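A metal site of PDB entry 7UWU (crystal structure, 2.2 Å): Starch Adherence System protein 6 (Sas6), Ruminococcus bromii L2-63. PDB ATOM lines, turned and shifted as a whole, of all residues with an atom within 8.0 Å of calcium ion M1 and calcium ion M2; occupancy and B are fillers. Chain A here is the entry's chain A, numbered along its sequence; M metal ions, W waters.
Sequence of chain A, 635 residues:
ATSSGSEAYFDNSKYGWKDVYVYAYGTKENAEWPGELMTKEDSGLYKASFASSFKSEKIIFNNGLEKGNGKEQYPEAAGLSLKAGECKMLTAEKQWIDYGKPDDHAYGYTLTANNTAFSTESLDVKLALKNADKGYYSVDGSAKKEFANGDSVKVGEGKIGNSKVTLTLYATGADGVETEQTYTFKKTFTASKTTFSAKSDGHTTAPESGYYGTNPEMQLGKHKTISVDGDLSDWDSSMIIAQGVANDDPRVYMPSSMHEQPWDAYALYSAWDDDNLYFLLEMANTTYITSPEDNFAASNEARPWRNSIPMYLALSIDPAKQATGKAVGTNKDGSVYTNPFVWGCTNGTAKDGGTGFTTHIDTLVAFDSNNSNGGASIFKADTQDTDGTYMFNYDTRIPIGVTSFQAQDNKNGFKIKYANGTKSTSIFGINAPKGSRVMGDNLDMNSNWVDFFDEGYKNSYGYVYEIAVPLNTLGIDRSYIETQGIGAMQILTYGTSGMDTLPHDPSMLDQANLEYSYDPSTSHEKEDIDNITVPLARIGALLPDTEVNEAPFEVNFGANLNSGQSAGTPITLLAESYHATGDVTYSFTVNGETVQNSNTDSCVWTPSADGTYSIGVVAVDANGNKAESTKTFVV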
ATOM      1  N   PRO A 250      20.680 -17.973 -10.699  1.00  0.00           N
ATOM      2  CA  PRO A 250      20.026 -16.652 -10.568  1.00  0.00           C
ATOM      3  C   PRO A 250      18.513 -16.693 -10.494  1.00  0.00           C
ATOM      4  O   PRO A 250      17.923 -15.875  -9.772  1.00  0.00           O
ATOM      5  CB  PRO A 250      20.501 -15.906 -11.832  1.00  0.00           C
ATOM      6  CG  PRO A 250      21.851 -16.486 -12.104  1.00  0.00           C
ATOM      7  CD  PRO A 250      21.784 -17.945 -11.685  1.00  0.00           C
ATOM      8  N   GLY A 353      25.599  -9.307 -22.645  1.00  0.00           N
ATOM      9  CA  GLY A 353      26.153  -9.997 -21.499  1.00  0.00           C
ATOM     10  C   GLY A 353      27.486 -10.673 -21.798  1.00  0.00           C
ATOM     11  O   GLY A 353      27.889 -10.853 -22.945  1.00  0.00           O
ATOM     12  N   GLY A 354      28.145 -11.054 -20.720  1.00  0.00           N
ATOM     13  CA  GLY A 354      29.442 -11.702 -20.827  1.00  0.00           C
ATOM     14  C   GLY A 354      30.076 -11.784 -19.459  1.00  0.00           C
ATOM     15  O   GLY A 354      29.586 -11.220 -18.478  1.00  0.00           O
ATOM     16  N   THR A 355      31.184 -12.535 -19.406  1.00  0.00           N
ATOM     17  CA  THR A 355      31.944 -12.692 -18.175  1.00  0.00           C
ATOM     18  C   THR A 355      33.381 -12.245 -18.419  1.00  0.00           C
ATOM     19  O   THR A 355      34.030 -12.748 -19.341  1.00  0.00           O
ATOM     20  CB  THR A 355      31.903 -14.142 -17.672  1.00  0.00           C
ATOM     21  OG1 THR A 355      30.544 -14.510 -17.413  1.00  0.00           O
ATOM     22  CG2 THR A 355      32.692 -14.279 -16.386  1.00  0.00           C
ATOM     23  N   LEU A 492      29.033 -21.318 -16.515  1.00  0.00           N
ATOM     24  CA  LEU A 492      27.800 -21.670 -17.199  1.00  0.00           C
ATOM     25  C   LEU A 492      27.095 -20.387 -17.619  1.00  0.00           C
ATOM     26  O   LEU A 492      27.130 -19.383 -16.901  1.00  0.00           O
ATOM     27  CB  LEU A 492      26.866 -22.502 -16.320  1.00  0.00           C
ATOM     28  CG  LEU A 492      27.310 -23.905 -15.895  1.00  0.00           C
ATOM     29  CD1 LEU A 492      26.225 -24.598 -15.083  1.00  0.00           C
ATOM     30  CD2 LEU A 492      27.688 -24.741 -17.102  1.00  0.00           C
ATOM     31  N   THR A 493      26.447 -20.425 -18.772  1.00  0.00           N
ATOM     32  CA  THR A 493      25.713 -19.272 -19.280  1.00  0.00           C
ATOM     33  C   THR A 493      24.287 -19.700 -19.622  1.00  0.00           C
ATOM     34  O   THR A 493      23.951 -20.887 -19.623  1.00  0.00           O
ATOM     35  CB  THR A 493      26.391 -18.670 -20.523  1.00  0.00           C
ATOM     36  OG1 THR A 493      25.907 -19.359 -21.694  1.00  0.00           O
ATOM     37  CG2 THR A 493      27.931 -18.764 -20.445  1.00  0.00           C
ATOM     38  N   TYR A 494      23.456 -18.710 -19.926  1.00  0.00           N
ATOM     39  CA  TYR A 494      22.189 -18.946 -20.608  1.00  0.00           C
ATOM     40  C   TYR A 494      22.185 -18.240 -21.951  1.00  0.00           C
ATOM     41  O   TYR A 494      21.225 -17.549 -22.321  1.00  0.00           O
ATOM     42  CB  TYR A 494      21.004 -18.502 -19.756  1.00  0.00           C
ATOM     43  CG  TYR A 494      19.689 -19.145 -20.139  1.00  0.00           C
ATOM     44  CD1 TYR A 494      19.630 -20.053 -21.192  1.00  0.00           C
ATOM     45  CD2 TYR A 494      18.514 -18.851 -19.458  1.00  0.00           C
ATOM     46  CE1 TYR A 494      18.441 -20.642 -21.559  1.00  0.00           C
ATOM     47  CE2 TYR A 494      17.316 -19.447 -19.818  1.00  0.00           C
ATOM     48  CZ  TYR A 494      17.288 -20.343 -20.871  1.00  0.00           C
ATOM     49  OH  TYR A 494      16.118 -20.945 -21.254  1.00  0.00           O
ATOM     50  N   THR A 496      24.764 -15.845 -23.018  1.00  0.00           N
ATOM     51  CA  THR A 496      25.872 -14.892 -23.051  1.00  0.00           C
ATOM     52  C   THR A 496      26.517 -14.713 -21.661  1.00  0.00           C
ATOM     53  O   THR A 496      27.582 -15.269 -21.389  1.00  0.00           O
ATOM     54  CB  THR A 496      25.408 -13.545 -23.574  1.00  0.00           C
ATOM     55  OG1 THR A 496      24.220 -13.154 -22.867  1.00  0.00           O
ATOM     56  CG2 THR A 496      25.106 -13.630 -25.073  1.00  0.00           C
ATOM     57  N   SER A 497      25.859 -13.929 -20.807  1.00  0.00           N
ATOM     58  CA  SER A 497      26.320 -13.685 -19.449  1.00  0.00           C
ATOM     59  C   SER A 497      26.446 -14.990 -18.652  1.00  0.00           C
ATOM     60  O   SER A 497      25.737 -15.974 -18.892  1.00  0.00           O
ATOM     61  CB  SER A 497      25.336 -12.748 -18.740  1.00  0.00           C
ATOM     62  OG  SER A 497      25.878 -12.220 -17.567  1.00  0.00           O
ATOM     63  N   GLY A 498      27.360 -14.999 -17.691  1.00  0.00           N
ATOM     64  CA  GLY A 498      27.429 -16.124 -16.777  1.00  0.00           C
ATOM     65  C   GLY A 498      26.181 -16.222 -15.900  1.00  0.00           C
ATOM     66  O   GLY A 498      25.427 -15.273 -15.716  1.00  0.00           O
ATOM     67  N   MET A 499      25.978 -17.433 -15.350  1.00  0.00           N
ATOM     68  CA  MET A 499      24.923 -17.711 -14.386  1.00  0.00           C
ATOM     69  C   MET A 499      25.447 -18.385 -13.142  1.00  0.00           C
ATOM     70  O   MET A 499      24.964 -18.122 -12.044  1.00  0.00           O
ATOM     71  CB  MET A 499      23.826 -18.603 -14.990  1.00  0.00           C
ATOM     72  CG  MET A 499      23.229 -18.076 -16.285  1.00  0.00           C
ATOM     73  SD  MET A 499      21.962 -16.862 -15.978  1.00  0.00           S
ATOM     74  CE  MET A 499      20.475 -17.895 -15.879  1.00  0.00           C
ATOM     75  N   ASP A 500      26.433 -19.267 -13.284  1.00  0.00           N
ATOM     76  CA  ASP A 500      26.946 -20.064 -12.184  1.00  0.00           C
ATOM     77  C   ASP A 500      28.388 -20.397 -12.525  1.00  0.00           C
ATOM     78  O   ASP A 500      28.734 -20.563 -13.700  1.00  0.00           O
ATOM     79  CB  ASP A 500      26.089 -21.332 -11.986  1.00  0.00           C
ATOM     80  CG  ASP A 500      26.264 -21.982 -10.601  1.00  0.00           C
ATOM     81  OD1 ASP A 500      27.249 -21.675  -9.900  1.00  0.00           O
ATOM     82  OD2 ASP A 500      25.412 -22.830 -10.238  1.00  0.00           O
ATOM     83  N   ASP A 505      31.534 -17.689  -7.973  1.00  0.00           N
ATOM     84  CA  ASP A 505      31.907 -16.260  -7.870  1.00  0.00           C
ATOM     85  C   ASP A 505      30.695 -15.379  -7.560  1.00  0.00           C
ATOM     86  O   ASP A 505      29.636 -15.563  -8.177  1.00  0.00           O
ATOM     87  CB  ASP A 505      32.576 -15.778  -9.172  1.00  0.00           C
ATOM     88  CG  ASP A 505      33.113 -14.345  -9.066  1.00  0.00           C
ATOM     89  OD1 ASP A 505      32.282 -13.399  -9.152  1.00  0.00           O
ATOM     90  OD2 ASP A 505      34.352 -14.180  -8.921  1.00  0.00           O
ATOM     91  N   PRO A 506      30.804 -14.409  -6.620  1.00  0.00           N
ATOM     92  CA  PRO A 506      29.623 -13.599  -6.266  1.00  0.00           C
ATOM     93  C   PRO A 506      29.084 -12.767  -7.413  1.00  0.00           C
ATOM     94  O   PRO A 506      27.920 -12.355  -7.352  1.00  0.00           O
ATOM     95  CB  PRO A 506      30.132 -12.700  -5.127  1.00  0.00           C
ATOM     96  CG  PRO A 506      31.582 -12.649  -5.306  1.00  0.00           C
ATOM     97  CD  PRO A 506      31.986 -14.008  -5.853  1.00  0.00           C
ATOM     98  N   SER A 507      29.872 -12.511  -8.457  1.00  0.00           N
ATOM     99  CA  SER A 507      29.302 -11.720  -9.544  1.00  0.00           C
ATOM    100  C   SER A 507      28.245 -12.514 -10.314  1.00  0.00           C
ATOM    101  O   SER A 507      27.527 -11.933 -11.145  1.00  0.00           O
ATOM    102  CB  SER A 507      30.420 -11.174 -10.457  1.00  0.00           C
ATOM    103  OG  SER A 507      30.891 -12.046 -11.478  1.00  0.00           O
ATOM    104  N   MET A 508      28.053 -13.790  -9.980  1.00  0.00           N
ATOM    105  CA  MET A 508      26.981 -14.568 -10.583  1.00  0.00           C
ATOM    106  C   MET A 508      25.608 -14.196 -10.024  1.00  0.00           C
ATOM    107  O   MET A 508      24.570 -14.552 -10.600  1.00  0.00           O
ATOM    108  CB  MET A 508      27.232 -16.057 -10.348  1.00  0.00           C
ATOM    109  CG  MET A 508      28.388 -16.620 -11.149  1.00  0.00           C
ATOM    110  SD  MET A 508      28.331 -16.354 -12.930  1.00  0.00           S
ATOM    111  CE  MET A 508      29.754 -15.305 -13.239  1.00  0.00           C
ATOM    112  N   LEU A 509      25.587 -13.495  -8.882  1.00  0.00           N
ATOM    113  CA  LEU A 509      24.350 -13.208  -8.170  1.00  0.00           C
ATOM    114  C   LEU A 509      24.263 -11.762  -7.720  1.00  0.00           C
ATOM    115  O   LEU A 509      23.310 -11.399  -7.011  1.00  0.00           O
ATOM    116  CB  LEU A 509      24.203 -14.160  -6.947  1.00  0.00           C
ATOM    117  CG  LEU A 509      24.098 -15.664  -7.257  1.00  0.00           C
ATOM    118  CD1 LEU A 509      24.103 -16.506  -5.961  1.00  0.00           C
ATOM    119  CD2 LEU A 509      22.855 -15.940  -8.073  1.00  0.00           C
ATOM    120  N   ASP A 510      25.231 -10.912  -8.097  1.00  0.00           N
ATOM    121  CA  ASP A 510      25.214  -9.517  -7.671  1.00  0.00           C
ATOM    122  C   ASP A 510      24.031  -8.756  -8.256  1.00  0.00           C
ATOM    123  O   ASP A 510      23.687  -7.690  -7.732  1.00  0.00           O
ATOM    124  CB  ASP A 510      26.536  -8.815  -8.011  1.00  0.00           C
ATOM    125  CG  ASP A 510      26.805  -8.719  -9.511  1.00  0.00           C
ATOM    126  OD1 ASP A 510      26.341  -9.589 -10.293  1.00  0.00           O
ATOM    127  OD2 ASP A 510      27.498  -7.763  -9.926  1.00  0.00           O
ATOM    128  N   GLN A 511      23.386  -9.281  -9.292  1.00  0.00           N
ATOM    129  CA  GLN A 511      22.189  -8.672  -9.856  1.00  0.00           C
ATOM    130  C   GLN A 511      21.066  -9.688 -10.048  1.00  0.00           C
ATOM    131  O   GLN A 511      20.152  -9.457 -10.846  1.00  0.00           O
ATOM    132  CB  GLN A 511      22.532  -7.950 -11.156  1.00  0.00           C
ATOM    133  CG  GLN A 511      23.845  -7.147 -11.063  1.00  0.00           C
ATOM    134  CD  GLN A 511      23.982  -6.076 -12.149  1.00  0.00           C
ATOM    135  OE1 GLN A 511      24.383  -6.359 -13.276  1.00  0.00           O
ATOM    136  NE2 GLN A 511      23.659  -4.838 -11.800  1.00  0.00           N
ATOM    137  N   ALA A 512      21.084 -10.802  -9.297  1.00  0.00           N
ATOM    138  CA  ALA A 512      20.173 -11.918  -9.577  1.00  0.00           C
ATOM    139  C   ALA A 512      18.697 -11.536  -9.485  1.00  0.00           C
ATOM    140  O   ALA A 512      17.868 -12.098 -10.217  1.00  0.00           O
ATOM    141  CB  ALA A 512      20.477 -13.081  -8.641  1.00  0.00           C
ATOM    142  N   SER A 523      15.568 -13.337 -14.640  1.00  0.00           N
ATOM    143  CA  SER A 523      16.638 -12.606 -14.001  1.00  0.00           C
ATOM    144  C   SER A 523      17.517 -11.868 -15.014  1.00  0.00           C
ATOM    145  O   SER A 523      17.828 -12.359 -16.089  1.00  0.00           O
ATOM    146  CB  SER A 523      17.534 -13.539 -13.181  1.00  0.00           C
ATOM    147  OG  SER A 523      18.651 -12.832 -12.698  1.00  0.00           O
ATOM    148  N   HIS A 524      17.958 -10.684 -14.597  1.00  0.00           N
ATOM    149  CA  HIS A 524      18.909  -9.902 -15.380  1.00  0.00           C
ATOM    150  C   HIS A 524      20.258 -10.609 -15.550  1.00  0.00           C
ATOM    151  O   HIS A 524      20.954 -10.342 -16.539  1.00  0.00           O
ATOM    152  CB  HIS A 524      19.038  -8.518 -14.716  1.00  0.00           C
ATOM    153  CG  HIS A 524      19.900  -7.542 -15.464  1.00  0.00           C
ATOM    154  ND1 HIS A 524      19.664  -7.191 -16.776  1.00  0.00           N
ATOM    155  CD2 HIS A 524      20.961  -6.792 -15.069  1.00  0.00           C
ATOM    156  CE1 HIS A 524      20.558  -6.300 -17.162  1.00  0.00           C
ATOM    157  NE2 HIS A 524      21.351  -6.046 -16.138  1.00  0.00           N
ATOM    158  N   GLU A 525      20.635 -11.536 -14.648  1.00  0.00           N
ATOM    159  CA  GLU A 525      21.946 -12.172 -14.749  1.00  0.00           C
ATOM    160  C   GLU A 525      22.179 -12.860 -16.084  1.00  0.00           C
ATOM    161  O   GLU A 525      23.327 -13.195 -16.396  1.00  0.00           O
ATOM    162  CB  GLU A 525      22.156 -13.198 -13.617  1.00  0.00           C
ATOM    163  CG  GLU A 525      22.574 -12.600 -12.266  1.00  0.00           C
ATOM    164  CD  GLU A 525      23.984 -12.001 -12.238  1.00  0.00           C
ATOM    165  OE1 GLU A 525      24.791 -12.294 -13.147  1.00  0.00           O
ATOM    166  OE2 GLU A 525      24.282 -11.228 -11.300  1.00  0.00           O
ATOM    167  N   LYS A 526      21.138 -13.100 -16.892  1.00  0.00           N
ATOM    168  CA  LYS A 526      21.328 -13.665 -18.217  1.00  0.00           C
ATOM    169  C   LYS A 526      22.024 -12.703 -19.170  1.00  0.00           C
ATOM    170  O   LYS A 526      22.586 -13.160 -20.179  1.00  0.00           O
ATOM    171  CB  LYS A 526      19.977 -14.062 -18.828  1.00  0.00           C
ATOM    172  CG  LYS A 526      19.170 -15.000 -17.961  1.00  0.00           C
ATOM    173  CD  LYS A 526      17.983 -15.559 -18.716  1.00  0.00           C
ATOM    174  CE  LYS A 526      16.707 -14.759 -18.416  1.00  0.00           C
ATOM    175  NZ  LYS A 526      15.547 -15.203 -19.244  1.00  0.00           N
ATOM    176  N   GLU A 527      21.997 -11.402 -18.885  1.00  0.00           N
ATOM    177  CA  GLU A 527      22.407 -10.405 -19.867  1.00  0.00           C
ATOM    178  C   GLU A 527      23.407  -9.393 -19.315  1.00  0.00           C
ATOM    179  O   GLU A 527      23.842  -8.520 -20.068  1.00  0.00           O
ATOM    180  CB  GLU A 527      21.175  -9.652 -20.416  1.00  0.00           C
ATOM    181  CG  GLU A 527      20.365  -8.900 -19.309  1.00  0.00           C
ATOM    182  CD  GLU A 527      19.198  -8.021 -19.811  1.00  0.00           C
ATOM    183  OE1 GLU A 527      19.017  -7.807 -21.035  1.00  0.00           O
ATOM    184  OE2 GLU A 527      18.439  -7.554 -18.952  1.00  0.00           O
ATOM    185  N   ASP A 528      23.771  -9.462 -18.035  1.00  0.00           N
ATOM    186  CA  ASP A 528      24.683  -8.468 -17.472  1.00  0.00           C
ATOM    187  C   ASP A 528      26.137  -8.890 -17.692  1.00  0.00           C
ATOM    188  O   ASP A 528      26.437  -9.904 -18.320  1.00  0.00           O
ATOM    189  CB  ASP A 528      24.392  -8.246 -15.986  1.00  0.00           C
ATOM    190  CG  ASP A 528      24.759  -9.447 -15.118  1.00  0.00           C
ATOM    191  OD1 ASP A 528      24.829 -10.572 -15.666  1.00  0.00           O
ATOM    192  OD2 ASP A 528      24.959  -9.269 -13.897  1.00  0.00           O
ATOM    193  N   ILE A 529      27.045  -8.072 -17.149  1.00  0.00           N
ATOM    194  CA  ILE A 529      28.487  -8.258 -17.304  1.00  0.00           C
ATOM    195  C   ILE A 529      29.031  -8.731 -15.968  1.00  0.00           C
ATOM    196  O   ILE A 529      28.961  -8.015 -14.968  1.00  0.00           O
ATOM    197  CB  ILE A 529      29.168  -6.953 -17.758  1.00  0.00           C
ATOM    198  CG1 ILE A 529      28.650  -6.542 -19.125  1.00  0.00           C
ATOM    199  CG2 ILE A 529      30.693  -7.090 -17.785  1.00  0.00           C
ATOM    200  CD1 ILE A 529      29.645  -5.739 -19.923  1.00  0.00           C
ATOM    201  N   ASP A 530      29.568  -9.943 -15.956  1.00  0.00           N
ATOM    202  CA  ASP A 530      30.162 -10.528 -14.763  1.00  0.00           C
ATOM    203  C   ASP A 530      31.662 -10.279 -14.776  1.00  0.00           C
ATOM    204  O   ASP A 530      32.264 -10.006 -15.817  1.00  0.00           O
ATOM    205  CB  ASP A 530      29.853 -12.033 -14.695  1.00  0.00           C
ATOM    206  CG  ASP A 530      28.339 -12.318 -14.670  1.00  0.00           C
ATOM    207  OD1 ASP A 530      27.601 -11.524 -14.075  1.00  0.00           O
ATOM    208  OD2 ASP A 530      27.892 -13.337 -15.251  1.00  0.00           O
ATOM    209  N   ASN A 531      32.270 -10.362 -13.608  1.00  0.00           N
ATOM    210  CA  ASN A 531      33.707 -10.105 -13.493  1.00  0.00           C
ATOM    211  C   ASN A 531      34.241 -11.002 -12.397  1.00  0.00           C
ATOM    212  O   ASN A 531      33.861 -10.839 -11.234  1.00  0.00           O
ATOM    213  CB  ASN A 531      33.971  -8.630 -13.198  1.00  0.00           C
ATOM    214  CG  ASN A 531      35.358  -8.407 -12.636  1.00  0.00           C
ATOM    215  OD1 ASN A 531      36.310  -9.018 -13.097  1.00  0.00           O
ATOM    216  ND2 ASN A 531      35.477  -7.524 -11.639  1.00  0.00           N
HETATM  217 CA    CA M   1      25.499 -12.866 -15.201  1.00  0.00          CA
HETATM  218 CA    CA M   2      26.279 -10.389 -12.438  1.00  0.00          CA
HETATM  219  O   HOH W   1      27.984  -8.637 -12.405  1.00  0.00           O
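O of Asp 528 lies within hydrogen-bond range of N of Gly 354. The side-chain hydroxyl of Ser 507 lies within hydrogen-bond range of the backbone NH of Asn 531, at 3.0 Å. The side-chain carboxylate (OD2) of Asp 528 lies close to the side-chain amide oxygen (OE1) of Gln 511 (3.0 Å). N of Glu 525 is in hydrogen-bond range of OG of Ser 523. The backbone carbonyl oxygen (O) of Gly 354 sits at hydrogen-bond distance from the backbone NH (N) of Asp 530, at 2.8 Å. N of Gly 498 sits at hydrogen-bond distance from OG1 of Thr 355. N of Ser 497 lies close to O of Lys 526, at 3.4 Å. The side-chain carboxylate (OD1) of Asp 505 lies within hydrogen-bond range of the backbone NH (N) of Ser 507 (2.7 Å).
Of the 29 residues printed, 5 come within 4 Å of calcium ion M1. The nearest printed residue that does not touch calcium ion M1 is Met 499 (4.6 Å).
Of the 29 residues printed, 5 come within 4 Å of calcium ion M2. Along chain A the residues within 4 Å of calcium ion M2 span positions 507 to 530.
Calcium ion M1 is bound by the side-chain carboxylate (OE1) of Glu 525, the side-chain carboxylate (OD1) of Asp 528, the side-chain carboxylate (OD2) of Asp 530, the backbone carbonyl oxygen (O) of Gly 498, the side-chain hydroxyl (OG) of Ser 497, the backbone carbonyl oxygen (O) of Glu 525 and the side-chain carboxylate (OD1) of Asp 530.
Calcium ion M2 is bound by the side-chain carboxylate (OD2) of Asp 528 (2.3 Å), the side-chain carboxylate (OD1) of Asp 510 (2.3 Å), the backbone carbonyl oxygen (O) of Ser 507 (2.4 Å), the side-chain carboxylate (OD1) of Asp 530 (2.4 Å), water W1 (2.4 Å), the side-chain carboxylate (OE2) of Glu 525 (2.4 Å) and the side-chain carboxylate (OE1) of Glu 525 (2.5 Å).
Water W1 lies within hydrogen-bond range of the side-chain carboxylate of Asp 510 and the backbone carbonyl oxygen of Ile 529.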
